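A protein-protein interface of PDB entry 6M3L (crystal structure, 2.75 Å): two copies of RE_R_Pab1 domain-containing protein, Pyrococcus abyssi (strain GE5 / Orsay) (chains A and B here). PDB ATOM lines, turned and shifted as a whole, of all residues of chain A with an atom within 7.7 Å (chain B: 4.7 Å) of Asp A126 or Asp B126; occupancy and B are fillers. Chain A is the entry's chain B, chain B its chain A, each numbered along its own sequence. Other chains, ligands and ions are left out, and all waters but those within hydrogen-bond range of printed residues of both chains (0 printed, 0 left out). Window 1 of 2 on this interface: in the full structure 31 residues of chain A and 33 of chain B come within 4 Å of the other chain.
The side-chain carboxylate (OE2) of Glu A125 is in salt-bridge range of the guanidinium group (NH2) of Arg B110 (3.0 Å). The backbone NH (N) of Tyr B124 sits at hydrogen-bond distance from the backbone carbonyl oxygen (O) of Val A130, 2.7 Å away. The side-chain carboxylate (OE1) of Glu B125 is in salt-bridge range of the guanidinium group (NH2) of Arg A110, 2.9 Å away. N of Asp B126 lies within hydrogen-bond range of O of Tyr A128, at 2.7 Å. N of Asp A126 lies within hydrogen-bond range of O of Tyr B128 (2.6 Å). O of Val B130 is in hydrogen-bond range of N of Tyr A124. The backbone carbonyl oxygen of Asp A126 sits close to the backbone carbonyl oxygen of Asp B126.
The backbone carbonyl oxygen of Arg B110 sits at hydrogen-bond distance from the backbone NH of Val B127, 2.9 Å away. NH2 of Arg B111 is in salt-bridge range of OD2 of Asp B126 (2.7 Å). NE of Arg A110 lies within salt-bridge range of OE2 of Glu A112 (3.3 Å). The backbone carbonyl oxygen of Arg A110 sits at hydrogen-bond distance from the backbone NH of Val A127, 2.9 Å away. NE of Arg A111 lies within salt-bridge range of OD1 of Asp A126, 2.7 Å away. The backbone carbonyl oxygen (O) of Glu A125 lies within hydrogen-bond range of the backbone NH (N) of Glu A112 (2.6 Å).
Glu A125 touches Val B127. Asp A126 touches Val B127 (O to CA, 3.4 Å). Val A127 touches Glu B125 (CG1 to CB, 3.7 Å). O of Asp B126 touches CA of Val A127, 3.5 Å away. Tyr A128 touches Tyr B124 (O to O, 3.95 Å). Glu B125 touches Tyr A128 (CA to O, 3.4 Å). Tyr B128 touches Tyr A128 (CD2 to CD1, 3.9 Å). Tyr B124 touches Pro A129. Arg B111 touches Val A130 (NH2 to CG2, 3.6 Å). Asp B126 touches Val A130 (OD2 to CG1, 3.4 Å).
Asp A126 touches four residues of chain B. Of chain A, only Asp A126, Val A127, Tyr A128 and Val A130 come within 4 Å of Asp B126. Of the printed residues of chain B, Tyr A124 touches Val B130. Of the printed residues of chain B, Glu A125 touches Arg B110, Val B127 and Tyr B128. Of the printed residues of chain B, Val A127 touches Glu B125 (3.7 Å) and Asp B126 (3.5 Å). Of the printed residues of chain A, Tyr B124 touches Tyr A128, Pro A129 and Val A130. Of the printed residues of chain B, Tyr A128 touches Tyr B124 (3.95 Å), Glu B125 (3.4 Å), Asp B126 (2.7 Å) and Tyr B128 (3.9 Å). Ile A109 touches none of the printed residues of chain B. The nearest residue of chain A that does not touch Asp B126 is Pro A129 (4.9 Å).
Hydrophobic or aromatic side chains of chain A within 4 Å of the printed part of chain B: Tyr A124, Val A127, Tyr A128 and Val A130. Of the 8 printed residues of chain B, 8 touch a printed residue of chain A. Hydrophobic or aromatic side chains of chain B within 4 Å of the printed part of chain A: Tyr B124, Val B127, Tyr B128 and Val B130. Among the printed residues, 20 pairs touch across the chains.
Tyr A124 touches Val B130, and with the chains exchanged Val A130 touches Tyr B124. Glu A125 touches Val B127, and with the chains exchanged Val A127 touches Glu B125. Asp A126 touches Tyr B128, and with the chains exchanged Tyr A128 touches Asp B126. Tyr A128 touches Tyr B124, but with the chains exchanged Tyr A124 does not touch Tyr B128 (4.03 Å). Of the 20 pairs that touch across the chains among the printed residues, 18 have their exchanged pair printed and touching as well.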
ATOM      1  N   ILE A 109      19.942  -7.791  14.123  1.00  0.00           N
ATOM      2  CA  ILE A 109      20.723  -8.541  13.150  1.00  0.00           C
ATOM      3  C   ILE A 109      21.765  -7.601  12.571  1.00  0.00           C
ATOM      4  O   ILE A 109      21.430  -6.511  12.087  1.00  0.00           O
ATOM      5  CB  ILE A 109      19.842  -9.138  12.039  1.00  0.00           C
ATOM      6  CG1 ILE A 109      18.908 -10.206  12.611  1.00  0.00           C
ATOM      7  CG2 ILE A 109      20.708  -9.722  10.931  1.00  0.00           C
ATOM      8  CD1 ILE A 109      17.517  -9.718  12.891  1.00  0.00           C
ATOM      9  N   ARG A 110      23.029  -8.007  12.635  1.00  0.00           N
ATOM     10  CA  ARG A 110      24.132  -7.216  12.113  1.00  0.00           C
ATOM     11  C   ARG A 110      24.801  -7.970  10.975  1.00  0.00           C
ATOM     12  O   ARG A 110      25.107  -9.161  11.103  1.00  0.00           O
ATOM     13  CB  ARG A 110      25.142  -6.882  13.214  1.00  0.00           C
ATOM     14  CG  ARG A 110      25.496  -8.037  14.140  1.00  0.00           C
ATOM     15  CD  ARG A 110      26.435  -7.562  15.244  1.00  0.00           C
ATOM     16  NE  ARG A 110      27.190  -8.657  15.847  1.00  0.00           N
ATOM     17  CZ  ARG A 110      26.837  -9.290  16.962  1.00  0.00           C
ATOM     18  NH1 ARG A 110      25.727  -8.943  17.603  1.00  0.00           N
ATOM     19  NH2 ARG A 110      27.592 -10.272  17.436  1.00  0.00           N
ATOM     20  N   ARG A 111      25.005  -7.277   9.860  1.00  0.00           N
ATOM     21  CA  ARG A 111      25.799  -7.778   8.747  1.00  0.00           C
ATOM     22  C   ARG A 111      27.228  -7.299   8.960  1.00  0.00           C
ATOM     23  O   ARG A 111      27.510  -6.101   8.856  1.00  0.00           O
ATOM     24  CB  ARG A 111      25.243  -7.294   7.410  1.00  0.00           C
ATOM     25  CG  ARG A 111      26.102  -7.655   6.205  1.00  0.00           C
ATOM     26  CD  ARG A 111      25.264  -7.644   4.939  1.00  0.00           C
ATOM     27  NE  ARG A 111      24.287  -8.730   4.947  1.00  0.00           N
ATOM     28  CZ  ARG A 111      23.238  -8.800   4.135  1.00  0.00           C
ATOM     29  NH1 ARG A 111      23.017  -7.840   3.247  1.00  0.00           N
ATOM     30  NH2 ARG A 111      22.404  -9.828   4.213  1.00  0.00           N
ATOM     31  N   GLU A 112      28.124  -8.231   9.258  1.00  0.00           N
ATOM     32  CA  GLU A 112      29.511  -7.899   9.536  1.00  0.00           C
ATOM     33  C   GLU A 112      30.354  -8.059   8.279  1.00  0.00           C
ATOM     34  O   GLU A 112      30.304  -9.100   7.615  1.00  0.00           O
ATOM     35  CB  GLU A 112      30.065  -8.766  10.667  1.00  0.00           C
ATOM     36  CG  GLU A 112      30.361  -7.961  11.912  1.00  0.00           C
ATOM     37  CD  GLU A 112      30.413  -8.803  13.166  1.00  0.00           C
ATOM     38  OE1 GLU A 112      30.773  -9.996  13.081  1.00  0.00           O
ATOM     39  OE2 GLU A 112      30.085  -8.259  14.242  1.00  0.00           O
ATOM     40  N   SER A 113      31.115  -7.019   7.959  1.00  0.00           N
ATOM     41  CA  SER A 113      32.093  -7.112   6.889  1.00  0.00           C
ATOM     42  C   SER A 113      33.254  -7.990   7.325  1.00  0.00           C
ATOM     43  O   SER A 113      33.742  -7.892   8.455  1.00  0.00           O
ATOM     44  CB  SER A 113      32.597  -5.718   6.509  1.00  0.00           C
ATOM     45  OG  SER A 113      33.736  -5.790   5.671  1.00  0.00           O
ATOM     46  N   THR A 114      33.673  -8.881   6.434  1.00  0.00           N
ATOM     47  CA  THR A 114      34.940  -9.575   6.566  1.00  0.00           C
ATOM     48  C   THR A 114      35.813  -9.190   5.382  1.00  0.00           C
ATOM     49  O   THR A 114      35.319  -8.825   4.312  1.00  0.00           O
ATOM     50  CB  THR A 114      34.764 -11.098   6.625  1.00  0.00           C
ATOM     51  OG1 THR A 114      34.617 -11.618   5.299  1.00  0.00           O
ATOM     52  CG2 THR A 114      33.537 -11.462   7.444  1.00  0.00           C
ATOM     53  N   TYR A 124      30.471 -11.502   3.616  1.00  0.00           N
ATOM     54  CA  TYR A 124      29.990 -10.907   4.853  1.00  0.00           C
ATOM     55  C   TYR A 124      29.421 -12.003   5.747  1.00  0.00           C
ATOM     56  O   TYR A 124      29.301 -13.166   5.351  1.00  0.00           O
ATOM     57  CB  TYR A 124      28.921  -9.832   4.590  1.00  0.00           C
ATOM     58  CG  TYR A 124      29.375  -8.676   3.732  1.00  0.00           C
ATOM     59  CD1 TYR A 124      29.617  -7.429   4.290  1.00  0.00           C
ATOM     60  CD2 TYR A 124      29.550  -8.826   2.362  1.00  0.00           C
ATOM     61  CE1 TYR A 124      30.025  -6.362   3.508  1.00  0.00           C
ATOM     62  CE2 TYR A 124      29.962  -7.766   1.573  1.00  0.00           C
ATOM     63  CZ  TYR A 124      30.197  -6.538   2.152  1.00  0.00           C
ATOM     64  OH  TYR A 124      30.605  -5.484   1.369  1.00  0.00           O
ATOM     65  N   GLU A 125      29.061 -11.617   6.969  1.00  0.00           N
ATOM     66  CA  GLU A 125      28.424 -12.525   7.914  1.00  0.00           C
ATOM     67  C   GLU A 125      27.231 -11.835   8.557  1.00  0.00           C
ATOM     68  O   GLU A 125      27.352 -10.712   9.056  1.00  0.00           O
ATOM     69  CB  GLU A 125      29.409 -13.003   8.992  1.00  0.00           C
ATOM     70  CG  GLU A 125      30.434 -14.003   8.474  1.00  0.00           C
ATOM     71  CD  GLU A 125      31.265 -14.627   9.580  1.00  0.00           C
ATOM     72  OE1 GLU A 125      31.723 -13.886  10.474  1.00  0.00           O
ATOM     73  OE2 GLU A 125      31.447 -15.862   9.558  1.00  0.00           O
ATOM     74  N   ASP A 126      26.083 -12.504   8.532  1.00  0.00           N
ATOM     75  CA  ASP A 126      24.870 -12.023   9.180  1.00  0.00           C
ATOM     76  C   ASP A 126      24.729 -12.725  10.524  1.00  0.00           C
ATOM     77  O   ASP A 126      24.643 -13.957  10.577  1.00  0.00           O
ATOM     78  CB  ASP A 126      23.639 -12.287   8.312  1.00  0.00           C
ATOM     79  CG  ASP A 126      23.583 -11.393   7.084  1.00  0.00           C
ATOM     80  OD1 ASP A 126      24.475 -10.532   6.928  1.00  0.00           O
ATOM     81  OD2 ASP A 126      22.644 -11.556   6.278  1.00  0.00           O
ATOM     82  N   VAL A 127      24.699 -11.948  11.598  1.00  0.00           N
ATOM     83  CA  VAL A 127      24.751 -12.480  12.956  1.00  0.00           C
ATOM     84  C   VAL A 127      23.362 -12.343  13.571  1.00  0.00           C
ATOM     85  O   VAL A 127      22.953 -11.255  13.990  1.00  0.00           O
ATOM     86  CB  VAL A 127      25.814 -11.775  13.804  1.00  0.00           C
ATOM     87  CG1 VAL A 127      25.938 -12.447  15.157  1.00  0.00           C
ATOM     88  CG2 VAL A 127      27.154 -11.774  13.076  1.00  0.00           C
ATOM     89  N   TYR A 128      22.634 -13.462  13.638  1.00  0.00           N
ATOM     90  CA  TYR A 128      21.317 -13.555  14.258  1.00  0.00           C
ATOM     91  C   TYR A 128      21.457 -14.014  15.706  1.00  0.00           C
ATOM     92  O   TYR A 128      22.145 -15.007  15.971  1.00  0.00           O
ATOM     93  CB  TYR A 128      20.430 -14.523  13.488  1.00  0.00           C
ATOM     94  CG  TYR A 128      19.977 -13.988  12.151  1.00  0.00           C
ATOM     95  CD1 TYR A 128      20.869 -13.860  11.092  1.00  0.00           C
ATOM     96  CD2 TYR A 128      18.658 -13.604  11.947  1.00  0.00           C
ATOM     97  CE1 TYR A 128      20.462 -13.365   9.873  1.00  0.00           C
ATOM     98  CE2 TYR A 128      18.243 -13.107  10.728  1.00  0.00           C
ATOM     99  CZ  TYR A 128      19.149 -12.992   9.696  1.00  0.00           C
ATOM    100  OH  TYR A 128      18.742 -12.500   8.478  1.00  0.00           O
ATOM    101  N   PRO A 129      20.841 -13.322  16.657  1.00  0.00           N
ATOM    102  CA  PRO A 129      20.985 -13.714  18.064  1.00  0.00           C
ATOM    103  C   PRO A 129      19.806 -14.533  18.560  1.00  0.00           C
ATOM    104  O   PRO A 129      18.654 -14.185  18.286  1.00  0.00           O
ATOM    105  CB  PRO A 129      21.073 -12.363  18.782  1.00  0.00           C
ATOM    106  CG  PRO A 129      20.189 -11.459  17.938  1.00  0.00           C
ATOM    107  CD  PRO A 129      20.210 -11.997  16.516  1.00  0.00           C
ATOM    108  N   VAL A 130      20.061 -15.621  19.284  1.00  0.00           N
ATOM    109  CA  VAL A 130      18.991 -16.455  19.820  1.00  0.00           C
ATOM    110  C   VAL A 130      19.232 -16.701  21.305  1.00  0.00           C
ATOM    111  O   VAL A 130      20.377 -16.820  21.756  1.00  0.00           O
ATOM    112  CB  VAL A 130      18.846 -17.792  19.054  1.00  0.00           C
ATOM    113  CG1 VAL A 130      18.493 -17.537  17.597  1.00  0.00           C
ATOM    114  CG2 VAL A 130      20.112 -18.614  19.145  1.00  0.00           C
ATOM    115  N   ALA A 131      18.143 -16.761  22.064  1.00  0.00           N
ATOM    116  CA  ALA A 131      18.179 -17.031  23.493  1.00  0.00           C
ATOM    117  C   ALA A 131      17.542 -18.388  23.741  1.00  0.00           C
ATOM    118  O   ALA A 131      16.403 -18.625  23.325  1.00  0.00           O
ATOM    119  CB  ALA A 131      17.451 -15.941  24.278  1.00  0.00           C
ATOM    120  N   ILE A 143      13.963 -18.043  21.682  1.00  0.00           N
ATOM    121  CA  ILE A 143      13.482 -16.757  21.190  1.00  0.00           C
ATOM    122  C   ILE A 143      14.413 -16.329  20.066  1.00  0.00           C
ATOM    123  O   ILE A 143      15.627 -16.203  20.274  1.00  0.00           O
ATOM    124  CB  ILE A 143      13.436 -15.699  22.302  1.00  0.00           C
ATOM    125  CG1 ILE A 143      12.872 -16.311  23.584  1.00  0.00           C
ATOM    126  CG2 ILE A 143      12.601 -14.497  21.868  1.00  0.00           C
ATOM    127  CD1 ILE A 143      13.092 -15.472  24.812  1.00  0.00           C
ATOM    128  N   VAL A 144      13.852 -16.114  18.880  1.00  0.00           N
ATOM    129  CA  VAL A 144      14.632 -15.795  17.693  1.00  0.00           C
ATOM    130  C   VAL A 144      14.224 -14.423  17.179  1.00  0.00           C
ATOM    131  O   VAL A 144      13.122 -13.933  17.446  1.00  0.00           O
ATOM    132  CB  VAL A 144      14.463 -16.861  16.592  1.00  0.00           C
ATOM    133  CG1 VAL A 144      14.902 -18.221  17.103  1.00  0.00           C
ATOM    134  CG2 VAL A 144      13.024 -16.905  16.135  1.00  0.00           C
ATOM    135  N   HIS A 147      14.083  -9.574  10.954  1.00  0.00           N
ATOM    136  CA  HIS A 147      13.791  -8.222  10.503  1.00  0.00           C
ATOM    137  C   HIS A 147      12.289  -7.993  10.505  1.00  0.00           C
ATOM    138  O   HIS A 147      11.524  -8.823  10.002  1.00  0.00           O
ATOM    139  CB  HIS A 147      14.361  -7.993   9.103  1.00  0.00           C
ATOM    140  CG  HIS A 147      15.853  -7.886   9.070  1.00  0.00           C
ATOM    141  ND1 HIS A 147      16.519  -6.706   9.325  1.00  0.00           N
ATOM    142  CD2 HIS A 147      16.809  -8.810   8.816  1.00  0.00           C
ATOM    143  CE1 HIS A 147      17.821  -6.909   9.228  1.00  0.00           C
ATOM    144  NE2 HIS A 147      18.023  -8.177   8.921  1.00  0.00           N
ATOM    145  N   ARG B 110      26.990 -21.646  11.442  1.00  0.00           N
ATOM    146  CA  ARG B 110      27.424 -22.070  12.768  1.00  0.00           C
ATOM    147  C   ARG B 110      26.676 -21.298  13.850  1.00  0.00           C
ATOM    148  O   ARG B 110      26.310 -20.134  13.668  1.00  0.00           O
ATOM    149  CB  ARG B 110      28.930 -21.897  12.969  1.00  0.00           C
ATOM    150  CG  ARG B 110      29.366 -20.476  13.223  1.00  0.00           C
ATOM    151  CD  ARG B 110      30.852 -20.339  12.997  1.00  0.00           C
ATOM    152  NE  ARG B 110      31.291 -18.953  13.121  1.00  0.00           N
ATOM    153  CZ  ARG B 110      31.717 -18.228  12.093  1.00  0.00           C
ATOM    154  NH1 ARG B 110      31.740 -18.759  10.878  1.00  0.00           N
ATOM    155  NH2 ARG B 110      32.100 -16.972  12.272  1.00  0.00           N
ATOM    156  N   ARG B 111      26.430 -21.970  14.971  1.00  0.00           N
ATOM    157  CA  ARG B 111      25.882 -21.345  16.171  1.00  0.00           C
ATOM    158  C   ARG B 111      26.987 -21.136  17.203  1.00  0.00           C
ATOM    159  O   ARG B 111      27.552 -22.108  17.715  1.00  0.00           O
ATOM    160  CB  ARG B 111      24.746 -22.185  16.744  1.00  0.00           C
ATOM    161  CG  ARG B 111      24.364 -21.822  18.164  1.00  0.00           C
ATOM    162  CD  ARG B 111      22.998 -22.381  18.459  1.00  0.00           C
ATOM    163  NE  ARG B 111      22.037 -21.737  17.572  1.00  0.00           N
ATOM    164  CZ  ARG B 111      20.727 -21.946  17.600  1.00  0.00           C
ATOM    165  NH1 ARG B 111      20.202 -22.800  18.472  1.00  0.00           N
ATOM    166  NH2 ARG B 111      19.941 -21.304  16.746  1.00  0.00           N
ATOM    167  N   TYR B 124      22.996 -17.237  22.131  1.00  0.00           N
ATOM    168  CA  TYR B 124      23.797 -17.757  21.032  1.00  0.00           C
ATOM    169  C   TYR B 124      23.737 -16.781  19.862  1.00  0.00           C
ATOM    170  O   TYR B 124      22.813 -15.973  19.743  1.00  0.00           O
ATOM    171  CB  TYR B 124      23.300 -19.131  20.558  1.00  0.00           C
ATOM    172  CG  TYR B 124      23.512 -20.279  21.520  1.00  0.00           C
ATOM    173  CD1 TYR B 124      24.791 -20.724  21.837  1.00  0.00           C
ATOM    174  CD2 TYR B 124      22.428 -20.941  22.088  1.00  0.00           C
ATOM    175  CE1 TYR B 124      24.981 -21.781  22.705  1.00  0.00           C
ATOM    176  CE2 TYR B 124      22.613 -21.996  22.952  1.00  0.00           C
ATOM    177  CZ  TYR B 124      23.888 -22.412  23.261  1.00  0.00           C
ATOM    178  OH  TYR B 124      24.068 -23.473  24.123  1.00  0.00           O
ATOM    179  N   GLU B 125      24.744 -16.865  18.993  1.00  0.00           N
ATOM    180  CA  GLU B 125      24.812 -16.092  17.753  1.00  0.00           C
ATOM    181  C   GLU B 125      24.891 -17.040  16.562  1.00  0.00           C
ATOM    182  O   GLU B 125      25.890 -17.751  16.400  1.00  0.00           O
ATOM    183  CB  GLU B 125      26.008 -15.134  17.758  1.00  0.00           C
ATOM    184  CG  GLU B 125      26.263 -14.445  19.082  1.00  0.00           C
ATOM    185  CD  GLU B 125      26.886 -13.072  18.908  1.00  0.00           C
ATOM    186  OE1 GLU B 125      28.009 -12.995  18.370  1.00  0.00           O
ATOM    187  OE2 GLU B 125      26.248 -12.070  19.296  1.00  0.00           O
ATOM    188  N   ASP B 126      23.850 -17.051  15.730  1.00  0.00           N
ATOM    189  CA  ASP B 126      23.861 -17.819  14.490  1.00  0.00           C
ATOM    190  C   ASP B 126      24.484 -16.958  13.394  1.00  0.00           C
ATOM    191  O   ASP B 126      23.955 -15.891  13.064  1.00  0.00           O
ATOM    192  CB  ASP B 126      22.441 -18.225  14.101  1.00  0.00           C
ATOM    193  CG  ASP B 126      21.853 -19.277  15.029  1.00  0.00           C
ATOM    194  OD1 ASP B 126      22.506 -20.317  15.247  1.00  0.00           O
ATOM    195  OD2 ASP B 126      20.734 -19.058  15.544  1.00  0.00           O
ATOM    196  N   VAL B 127      25.586 -17.428  12.810  1.00  0.00           N
ATOM    197  CA  VAL B 127      26.368 -16.644  11.858  1.00  0.00           C
ATOM    198  C   VAL B 127      26.154 -17.229  10.464  1.00  0.00           C
ATOM    199  O   VAL B 127      26.557 -18.368  10.198  1.00  0.00           O
ATOM    200  CB  VAL B 127      27.855 -16.617  12.243  1.00  0.00           C
ATOM    201  CG1 VAL B 127      28.649 -15.845  11.215  1.00  0.00           C
ATOM    202  CG2 VAL B 127      28.030 -16.014  13.629  1.00  0.00           C
ATOM    203  N   TYR B 128      25.539 -16.433   9.566  1.00  0.00           N
ATOM    204  CA  TYR B 128      25.229 -16.803   8.184  1.00  0.00           C
ATOM    205  C   TYR B 128      26.076 -16.022   7.186  1.00  0.00           C
ATOM    206  O   TYR B 128      26.161 -14.791   7.288  1.00  0.00           O
ATOM    207  CB  TYR B 128      23.751 -16.572   7.876  1.00  0.00           C
ATOM    208  CG  TYR B 128      22.789 -17.485   8.601  1.00  0.00           C
ATOM    209  CD1 TYR B 128      22.216 -18.577   7.963  1.00  0.00           C
ATOM    210  CD2 TYR B 128      22.394 -17.207   9.901  1.00  0.00           C
ATOM    211  CE1 TYR B 128      21.315 -19.396   8.623  1.00  0.00           C
ATOM    212  CE2 TYR B 128      21.492 -18.015  10.565  1.00  0.00           C
ATOM    213  CZ  TYR B 128      20.956 -19.108   9.922  1.00  0.00           C
ATOM    214  OH  TYR B 128      20.060 -19.910  10.590  1.00  0.00           O
ATOM    215  N   VAL B 130      27.072 -14.298   3.541  1.00  0.00           N
ATOM    216  CA  VAL B 130      26.492 -13.737   2.327  1.00  0.00           C
ATOM    217  C   VAL B 130      27.602 -13.183   1.442  1.00  0.00           C
ATOM    218  O   VAL B 130      28.685 -12.819   1.914  1.00  0.00           O
ATOM    219  CB  VAL B 130      25.436 -12.642   2.611  1.00  0.00           C
ATOM    220  CG1 VAL B 130      24.440 -13.106   3.664  1.00  0.00           C
ATOM    221  CG2 VAL B 130      26.103 -11.338   3.024  1.00  0.00           C
